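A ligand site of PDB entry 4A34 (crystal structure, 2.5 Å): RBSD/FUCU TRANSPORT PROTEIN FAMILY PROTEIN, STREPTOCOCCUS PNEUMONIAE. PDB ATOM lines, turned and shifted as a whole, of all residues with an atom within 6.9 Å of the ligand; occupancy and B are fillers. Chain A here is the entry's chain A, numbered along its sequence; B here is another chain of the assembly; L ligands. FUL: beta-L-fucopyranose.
O3 of the ligand lies within hydrogen-bond range of N of Tyr 130 (2.8 Å). ND2 of Asn 132 lies within hydrogen-bond range of O2 of the ligand (2.7 Å). O3 of the ligand is in hydrogen-bond range of OD2 of Asp 30. O5 of the ligand is in hydrogen-bond range of ND1 of His 22 of chain B (2.5 Å). The side-chain hydroxyl (OH) of Tyr 112 sits at hydrogen-bond distance from an oxygen (O1) of the ligand, 2.9 Å away.
The backbone NH of Asn 32 sits close to the side-chain carboxylate of Asp 30, 3.1 Å away. The backbone NH (N) of Tyr 33 sits at hydrogen-bond distance from the side-chain carboxylate (OD1) of Asp 30 (3.2 Å). The side-chain carboxylate (OD2) of Asp 30 is in hydrogen-bond range of the backbone NH (N) of Tyr 130 (3.4 Å). N of Asp 30 lies within hydrogen-bond range of OD1 of Asn 132, 2.8 Å away. The side-chain hydroxyl of Tyr 130 lies within hydrogen-bond range of the side-chain carboxylate of Asp 80. The side-chain carboxylate (OD2) of Asp 80 lies within hydrogen-bond range of the side-chain hydroxyl (OH) of Tyr 66 of chain B, at 3.0 Å. N of Val 140 of chain B lies within hydrogen-bond range of OD1 of Asn 32, 2.9 Å away. OH of Tyr 112 lies within hydrogen-bond range of NE of Arg 108, 3.3 Å away.
O of Asn 32 touches O1 of the ligand, 3.7 Å away. CD1 of Tyr 33 touches O2 of the ligand (3.7 Å). CD of Pro 34 touches O1 of the ligand, at 3.8 Å. Leu 129 touches the ligand (CA to O3, 3.4 Å). Tyr 66 of chain B touches the ligand. CG2 of Val 139 of chain B touches O4 of the ligand, at 3.1 Å. Hydrophobic or aromatic side chains that line the ligand: Tyr 33, Pro 34, Tyr 112, Leu 129, Tyr 130, His 22 of chain B, Tyr 66 of chain B and Val 139 of chain B. Within 4 Å of the ligand: Asp 30, Asn 32, Tyr 33, Pro 34, Tyr 112, Leu 129, Tyr 130, Asn 132, His 22 of chain B, Tyr 66 of chain B and Val 139 of chain B. Along chain A the residues within 4 Å of the ligand span positions 30 to 132. The nearest printed residue that does not touch the ligand is Met 74 (4.1 Å).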
ATOM      1  N   ALA A  29      30.155  -0.056  -2.582  1.00  0.00           N
ATOM      2  CA  ALA A  29      28.931  -0.811  -2.817  1.00  0.00           C
ATOM      3  C   ALA A  29      28.475  -0.671  -4.263  1.00  0.00           C
ATOM      4  O   ALA A  29      28.576   0.409  -4.837  1.00  0.00           O
ATOM      5  CB  ALA A  29      27.831  -0.333  -1.875  1.00  0.00           C
ATOM      6  N   ASP A  30      27.974  -1.759  -4.824  1.00  0.00           N
ATOM      7  CA  ASP A  30      27.556  -1.743  -6.213  1.00  0.00           C
ATOM      8  C   ASP A  30      26.201  -1.055  -6.357  1.00  0.00           C
ATOM      9  O   ASP A  30      25.546  -0.738  -5.361  1.00  0.00           O
ATOM     10  CB  ASP A  30      27.595  -3.154  -6.834  1.00  0.00           C
ATOM     11  CG  ASP A  30      26.654  -4.139  -6.155  1.00  0.00           C
ATOM     12  OD1 ASP A  30      25.566  -3.768  -5.666  1.00  0.00           O
ATOM     13  OD2 ASP A  30      27.006  -5.328  -6.140  1.00  0.00           O
ATOM     14  N   ALA A  31      25.787  -0.805  -7.600  1.00  0.00           N
ATOM     15  CA  ALA A  31      24.554  -0.052  -7.856  1.00  0.00           C
ATOM     16  C   ALA A  31      23.289  -0.695  -7.279  1.00  0.00           C
ATOM     17  O   ALA A  31      22.254  -0.062  -7.250  1.00  0.00           O
ATOM     18  CB  ALA A  31      24.389   0.205  -9.347  1.00  0.00           C
ATOM     19  N   ASN A  32      23.369  -1.940  -6.828  1.00  0.00           N
ATOM     20  CA  ASN A  32      22.207  -2.622  -6.272  1.00  0.00           C
ATOM     21  C   ASN A  32      22.210  -2.727  -4.740  1.00  0.00           C
ATOM     22  O   ASN A  32      21.262  -3.276  -4.146  1.00  0.00           O
ATOM     23  CB  ASN A  32      22.022  -4.001  -6.903  1.00  0.00           C
ATOM     24  CG  ASN A  32      21.278  -3.938  -8.220  1.00  0.00           C
ATOM     25  OD1 ASN A  32      20.044  -3.950  -8.257  1.00  0.00           O
ATOM     26  ND2 ASN A  32      22.023  -3.896  -9.325  1.00  0.00           N
ATOM     27  N   TYR A  33      23.256  -2.214  -4.114  1.00  0.00           N
ATOM     28  CA  TYR A  33      23.381  -2.296  -2.665  1.00  0.00           C
ATOM     29  C   TYR A  33      22.439  -1.336  -1.925  1.00  0.00           C
ATOM     30  O   TYR A  33      22.195  -0.222  -2.397  1.00  0.00           O
ATOM     31  CB  TYR A  33      24.831  -2.063  -2.232  1.00  0.00           C
ATOM     32  CG  TYR A  33      25.129  -2.597  -0.850  1.00  0.00           C
ATOM     33  CD1 TYR A  33      25.526  -3.920  -0.683  1.00  0.00           C
ATOM     34  CD2 TYR A  33      24.988  -1.807   0.280  1.00  0.00           C
ATOM     35  CE1 TYR A  33      25.798  -4.430   0.588  1.00  0.00           C
ATOM     36  CE2 TYR A  33      25.249  -2.312   1.543  1.00  0.00           C
ATOM     37  CZ  TYR A  33      25.655  -3.632   1.689  1.00  0.00           C
ATOM     38  OH  TYR A  33      25.939  -4.134   2.928  1.00  0.00           O
ATOM     39  N   PRO A  34      21.881  -1.778  -0.777  1.00  0.00           N
ATOM     40  CA  PRO A  34      21.135  -0.897   0.121  1.00  0.00           C
ATOM     41  C   PRO A  34      22.071   0.047   0.896  1.00  0.00           C
ATOM     42  O   PRO A  34      22.170  -0.031   2.121  1.00  0.00           O
ATOM     43  CB  PRO A  34      20.453  -1.883   1.088  1.00  0.00           C
ATOM     44  CG  PRO A  34      21.289  -3.083   1.061  1.00  0.00           C
ATOM     45  CD  PRO A  34      21.787  -3.191  -0.351  1.00  0.00           C
ATOM     46  N   MET A  74      31.120 -10.179  -1.153  1.00  0.00           N
ATOM     47  CA  MET A  74      29.829 -10.784  -0.849  1.00  0.00           C
ATOM     48  C   MET A  74      29.681 -12.080  -1.649  1.00  0.00           C
ATOM     49  O   MET A  74      29.801 -12.098  -2.879  1.00  0.00           O
ATOM     50  CB  MET A  74      28.668  -9.818  -1.120  1.00  0.00           C
ATOM     51  CG  MET A  74      27.293 -10.395  -0.755  1.00  0.00           C
ATOM     52  SD  MET A  74      25.890  -9.390  -1.305  1.00  0.00           S
ATOM     53  CE  MET A  74      25.969  -8.012  -0.162  1.00  0.00           C
ATOM     54  N   ASN A  75      29.424 -13.169  -0.931  1.00  0.00           N
ATOM     55  CA  ASN A  75      29.262 -14.478  -1.539  1.00  0.00           C
ATOM     56  C   ASN A  75      27.946 -14.582  -2.284  1.00  0.00           C
ATOM     57  O   ASN A  75      26.993 -13.888  -1.951  1.00  0.00           O
ATOM     58  CB  ASN A  75      29.344 -15.582  -0.493  1.00  0.00           C
ATOM     59  CG  ASN A  75      29.915 -16.875  -1.055  1.00  0.00           C
ATOM     60  OD1 ASN A  75      30.083 -17.023  -2.268  1.00  0.00           O
ATOM     61  ND2 ASN A  75      30.225 -17.799  -0.164  1.00  0.00           N
ATOM     62  N   VAL A  77      24.441 -16.469  -3.635  1.00  0.00           N
ATOM     63  CA  VAL A  77      23.449 -17.478  -3.257  1.00  0.00           C
ATOM     64  C   VAL A  77      23.291 -18.407  -4.460  1.00  0.00           C
ATOM     65  O   VAL A  77      23.210 -17.930  -5.595  1.00  0.00           O
ATOM     66  CB  VAL A  77      22.089 -16.846  -2.894  1.00  0.00           C
ATOM     67  N   ASP A  80      23.462 -18.379  -8.402  1.00  0.00           N
ATOM     68  CA  ASP A  80      23.805 -17.186  -9.134  1.00  0.00           C
ATOM     69  C   ASP A  80      25.182 -17.398  -9.697  1.00  0.00           C
ATOM     70  O   ASP A  80      25.938 -18.249  -9.207  1.00  0.00           O
ATOM     71  CB  ASP A  80      23.790 -15.954  -8.234  1.00  0.00           C
ATOM     72  CG  ASP A  80      22.395 -15.442  -7.956  1.00  0.00           C
ATOM     73  OD1 ASP A  80      21.430 -16.022  -8.484  1.00  0.00           O
ATOM     74  OD2 ASP A  80      22.266 -14.458  -7.200  1.00  0.00           O
ATOM     75  N   ARG A 108      25.400 -12.838   2.159  1.00  0.00           N
ATOM     76  CA  ARG A 108      24.582 -11.642   2.050  1.00  0.00           C
ATOM     77  C   ARG A 108      24.265 -10.949   3.383  1.00  0.00           C
ATOM     78  O   ARG A 108      24.628  -9.796   3.594  1.00  0.00           O
ATOM     79  CB  ARG A 108      23.301 -11.994   1.286  1.00  0.00           C
ATOM     80  CG  ARG A 108      22.709 -10.867   0.457  1.00  0.00           C
ATOM     81  CD  ARG A 108      21.757 -11.413  -0.603  1.00  0.00           C
ATOM     82  NE  ARG A 108      20.544 -10.596  -0.724  1.00  0.00           N
ATOM     83  CZ  ARG A 108      19.380 -10.892  -0.147  1.00  0.00           C
ATOM     84  NH1 ARG A 108      19.258 -11.982   0.602  1.00  0.00           N
ATOM     85  NH2 ARG A 108      18.331 -10.096  -0.311  1.00  0.00           N
ATOM     86  N   TYR A 112      25.743  -7.353   4.975  1.00  0.00           N
ATOM     87  CA  TYR A 112      24.904  -6.204   5.348  1.00  0.00           C
ATOM     88  C   TYR A 112      25.212  -5.733   6.766  1.00  0.00           C
ATOM     89  O   TYR A 112      25.454  -4.555   6.995  1.00  0.00           O
ATOM     90  CB  TYR A 112      23.403  -6.533   5.251  1.00  0.00           C
ATOM     91  CG  TYR A 112      22.838  -6.784   3.855  1.00  0.00           C
ATOM     92  CD1 TYR A 112      23.334  -6.093   2.733  1.00  0.00           C
ATOM     93  CD2 TYR A 112      21.801  -7.697   3.656  1.00  0.00           C
ATOM     94  CE1 TYR A 112      22.813  -6.328   1.454  1.00  0.00           C
ATOM     95  CE2 TYR A 112      21.271  -7.935   2.373  1.00  0.00           C
ATOM     96  CZ  TYR A 112      21.778  -7.250   1.284  1.00  0.00           C
ATOM     97  OH  TYR A 112      21.261  -7.479   0.018  1.00  0.00           O
ATOM     98  N   GLU A 126      28.372   0.868 -10.118  1.00  0.00           N
ATOM     99  CA  GLU A 126      28.727  -0.463 -10.608  1.00  0.00           C
ATOM    100  C   GLU A 126      27.498  -1.325 -10.927  1.00  0.00           C
ATOM    101  O   GLU A 126      26.662  -1.556 -10.060  1.00  0.00           O
ATOM    102  CB  GLU A 126      29.632  -1.157  -9.578  1.00  0.00           C
ATOM    103  CG  GLU A 126      30.164  -2.491 -10.024  1.00  0.00           C
ATOM    104  CD  GLU A 126      30.850  -2.431 -11.367  1.00  0.00           C
ATOM    105  OE1 GLU A 126      31.938  -1.804 -11.468  1.00  0.00           O
ATOM    106  OE2 GLU A 126      30.301  -3.019 -12.320  1.00  0.00           O
ATOM    107  N   THR A 127      27.394  -1.787 -12.168  1.00  0.00           N
ATOM    108  CA  THR A 127      26.225  -2.562 -12.582  1.00  0.00           C
ATOM    109  C   THR A 127      26.395  -4.043 -12.330  1.00  0.00           C
ATOM    110  O   THR A 127      25.391  -4.754 -12.172  1.00  0.00           O
ATOM    111  CB  THR A 127      25.865  -2.375 -14.050  1.00  0.00           C
ATOM    112  OG1 THR A 127      27.001  -2.699 -14.859  1.00  0.00           O
ATOM    113  CG2 THR A 127      25.399  -0.944 -14.324  1.00  0.00           C
ATOM    114  N   SER A 128      27.635  -4.511 -12.302  1.00  0.00           N
ATOM    115  CA  SER A 128      27.930  -5.901 -11.962  1.00  0.00           C
ATOM    116  C   SER A 128      27.321  -6.284 -10.622  1.00  0.00           C
ATOM    117  O   SER A 128      27.374  -5.510  -9.653  1.00  0.00           O
ATOM    118  CB  SER A 128      29.433  -6.166 -11.905  1.00  0.00           C
ATOM    119  OG  SER A 128      29.702  -7.308 -11.089  1.00  0.00           O
ATOM    120  N   LEU A 129      26.751  -7.487 -10.569  1.00  0.00           N
ATOM    121  CA  LEU A 129      26.175  -8.034  -9.354  1.00  0.00           C
ATOM    122  C   LEU A 129      27.286  -8.550  -8.430  1.00  0.00           C
ATOM    123  O   LEU A 129      28.372  -8.879  -8.899  1.00  0.00           O
ATOM    124  CB  LEU A 129      25.188  -9.148  -9.690  1.00  0.00           C
ATOM    125  CG  LEU A 129      23.992  -8.812 -10.596  1.00  0.00           C
ATOM    126  CD1 LEU A 129      23.007  -9.981 -10.593  1.00  0.00           C
ATOM    127  CD2 LEU A 129      23.277  -7.531 -10.164  1.00  0.00           C
ATOM    128  N   TYR A 130      26.986  -8.602  -7.132  1.00  0.00           N
ATOM    129  CA  TYR A 130      27.918  -9.079  -6.096  1.00  0.00           C
ATOM    130  C   TYR A 130      29.270  -8.434  -6.208  1.00  0.00           C
ATOM    131  O   TYR A 130      30.295  -9.082  -6.005  1.00  0.00           O
ATOM    132  CB  TYR A 130      28.074 -10.613  -6.150  1.00  0.00           C
ATOM    133  CG  TYR A 130      26.792 -11.357  -5.812  1.00  0.00           C
ATOM    134  CD1 TYR A 130      26.446 -11.646  -4.488  1.00  0.00           C
ATOM    135  CD2 TYR A 130      25.916 -11.757  -6.821  1.00  0.00           C
ATOM    136  CE1 TYR A 130      25.266 -12.312  -4.181  1.00  0.00           C
ATOM    137  CE2 TYR A 130      24.733 -12.430  -6.526  1.00  0.00           C
ATOM    138  CZ  TYR A 130      24.412 -12.711  -5.214  1.00  0.00           C
ATOM    139  OH  TYR A 130      23.231 -13.368  -4.936  1.00  0.00           O
ATOM    140  N   ALA A 131      29.275  -7.140  -6.530  1.00  0.00           N
ATOM    141  CA  ALA A 131      30.516  -6.419  -6.760  1.00  0.00           C
ATOM    142  C   ALA A 131      30.954  -5.599  -5.535  1.00  0.00           C
ATOM    143  O   ALA A 131      31.927  -4.840  -5.583  1.00  0.00           O
ATOM    144  CB  ALA A 131      30.383  -5.536  -8.008  1.00  0.00           C
ATOM    145  N   ASN A 132      30.233  -5.790  -4.420  1.00  0.00           N
ATOM    146  CA  ASN A 132      30.501  -5.088  -3.163  1.00  0.00           C
ATOM    147  C   ASN A 132      31.828  -5.485  -2.547  1.00  0.00           C
ATOM    148  O   ASN A 132      32.202  -6.639  -2.606  1.00  0.00           O
ATOM    149  CB  ASN A 132      29.378  -5.354  -2.145  1.00  0.00           C
ATOM    150  CG  ASN A 132      28.004  -5.128  -2.734  1.00  0.00           C
ATOM    151  OD1 ASN A 132      27.677  -4.027  -3.165  1.00  0.00           O
ATOM    152  ND2 ASN A 132      27.183  -6.166  -2.758  1.00  0.00           N
ATOM    153  N   GLY B  21      17.927   0.164  -2.037  1.00  0.00           N
ATOM    154  CA  GLY B  21      18.716  -0.923  -2.599  1.00  0.00           C
ATOM    155  C   GLY B  21      17.943  -2.232  -2.527  1.00  0.00           C
ATOM    156  O   GLY B  21      16.809  -2.273  -2.054  1.00  0.00           O
ATOM    157  N   HIS B  22      18.576  -3.295  -2.993  1.00  0.00           N
ATOM    158  CA  HIS B  22      18.020  -4.640  -2.940  1.00  0.00           C
ATOM    159  C   HIS B  22      17.756  -5.037  -1.488  1.00  0.00           C
ATOM    160  O   HIS B  22      18.674  -5.058  -0.660  1.00  0.00           O
ATOM    161  CB  HIS B  22      19.009  -5.612  -3.598  1.00  0.00           C
ATOM    162  CG  HIS B  22      18.613  -7.048  -3.500  1.00  0.00           C
ATOM    163  ND1 HIS B  22      19.548  -8.058  -3.407  1.00  0.00           N
ATOM    164  CD2 HIS B  22      17.400  -7.647  -3.496  1.00  0.00           C
ATOM    165  CE1 HIS B  22      18.919  -9.224  -3.354  1.00  0.00           C
ATOM    166  NE2 HIS B  22      17.620  -9.003  -3.396  1.00  0.00           N
ATOM    167  N   GLY B  23      16.499  -5.338  -1.184  1.00  0.00           N
ATOM    168  CA  GLY B  23      16.104  -5.739   0.154  1.00  0.00           C
ATOM    169  C   GLY B  23      15.374  -4.669   0.952  1.00  0.00           C
ATOM    170  O   GLY B  23      14.646  -5.000   1.885  1.00  0.00           O
ATOM    171  N   TYR B  66      14.451 -12.803  -4.207  1.00  0.00           N
ATOM    172  CA  TYR B  66      15.210 -13.641  -3.280  1.00  0.00           C
ATOM    173  C   TYR B  66      14.502 -13.921  -1.952  1.00  0.00           C
ATOM    174  O   TYR B  66      15.097 -14.447  -1.022  1.00  0.00           O
ATOM    175  CB  TYR B  66      16.574 -13.023  -2.997  1.00  0.00           C
ATOM    176  CG  TYR B  66      17.488 -12.904  -4.203  1.00  0.00           C
ATOM    177  CD1 TYR B  66      17.226 -11.979  -5.225  1.00  0.00           C
ATOM    178  CD2 TYR B  66      18.649 -13.692  -4.317  1.00  0.00           C
ATOM    179  CE1 TYR B  66      18.069 -11.864  -6.324  1.00  0.00           C
ATOM    180  CE2 TYR B  66      19.502 -13.575  -5.413  1.00  0.00           C
ATOM    181  CZ  TYR B  66      19.204 -12.652  -6.406  1.00  0.00           C
ATOM    182  OH  TYR B  66      20.038 -12.531  -7.489  1.00  0.00           O
ATOM    183  N   GLY B 138      13.642  -5.356  -5.545  1.00  0.00           N
ATOM    184  CA  GLY B 138      14.465  -6.365  -6.189  1.00  0.00           C
ATOM    185  C   GLY B 138      15.741  -5.813  -6.799  1.00  0.00           C
ATOM    186  O   GLY B 138      16.102  -4.642  -6.571  1.00  0.00           O
ATOM    187  N   VAL B 139      16.416  -6.656  -7.569  1.00  0.00           N
ATOM    188  CA  VAL B 139      17.614  -6.283  -8.303  1.00  0.00           C
ATOM    189  C   VAL B 139      17.255  -5.770  -9.688  1.00  0.00           C
ATOM    190  O   VAL B 139      16.234  -6.156 -10.263  1.00  0.00           O
ATOM    191  CB  VAL B 139      18.608  -7.458  -8.368  1.00  0.00           C
ATOM    192  CG1 VAL B 139      19.728  -7.198  -9.373  1.00  0.00           C
ATOM    193  CG2 VAL B 139      19.200  -7.709  -6.983  1.00  0.00           C
ATOM    194  N   VAL B 140      18.082  -4.860 -10.210  1.00  0.00           N
ATOM    195  CA  VAL B 140      17.850  -4.233 -11.503  1.00  0.00           C
ATOM    196  C   VAL B 140      18.794  -4.774 -12.586  1.00  0.00           C
ATOM    197  O   VAL B 140      19.996  -4.956 -12.334  1.00  0.00           O
ATOM    198  CB  VAL B 140      17.988  -2.699 -11.387  1.00  0.00           C
ATOM    199  CG1 VAL B 140      18.425  -2.091 -12.719  1.00  0.00           C
ATOM    200  CG2 VAL B 140      16.685  -2.084 -10.910  1.00  0.00           C
HETATM  201  C1  FUL L   1      22.966  -7.260  -3.218  1.00  0.00           C
HETATM  202  C2  FUL L   1      23.737  -6.533  -4.338  1.00  0.00           C
HETATM  203  O2  FUL L   1      24.777  -5.725  -3.841  1.00  0.00           O
HETATM  204  C3  FUL L   1      24.335  -7.572  -5.274  1.00  0.00           C
HETATM  205  O3  FUL L   1      24.859  -6.957  -6.424  1.00  0.00           O
HETATM  206  C4  FUL L   1      23.263  -8.584  -5.676  1.00  0.00           C
HETATM  207  O4  FUL L   1      22.230  -7.879  -6.309  1.00  0.00           O
HETATM  208  C5  FUL L   1      22.687  -9.239  -4.431  1.00  0.00           C
HETATM  209  C6  FUL L   1      21.771 -10.406  -4.755  1.00  0.00           C
HETATM  210  O5  FUL L   1      22.024  -8.204  -3.728  1.00  0.00           O
HETATM  211  O1  FUL L   1      22.311  -6.353  -2.387  1.00  0.00           O
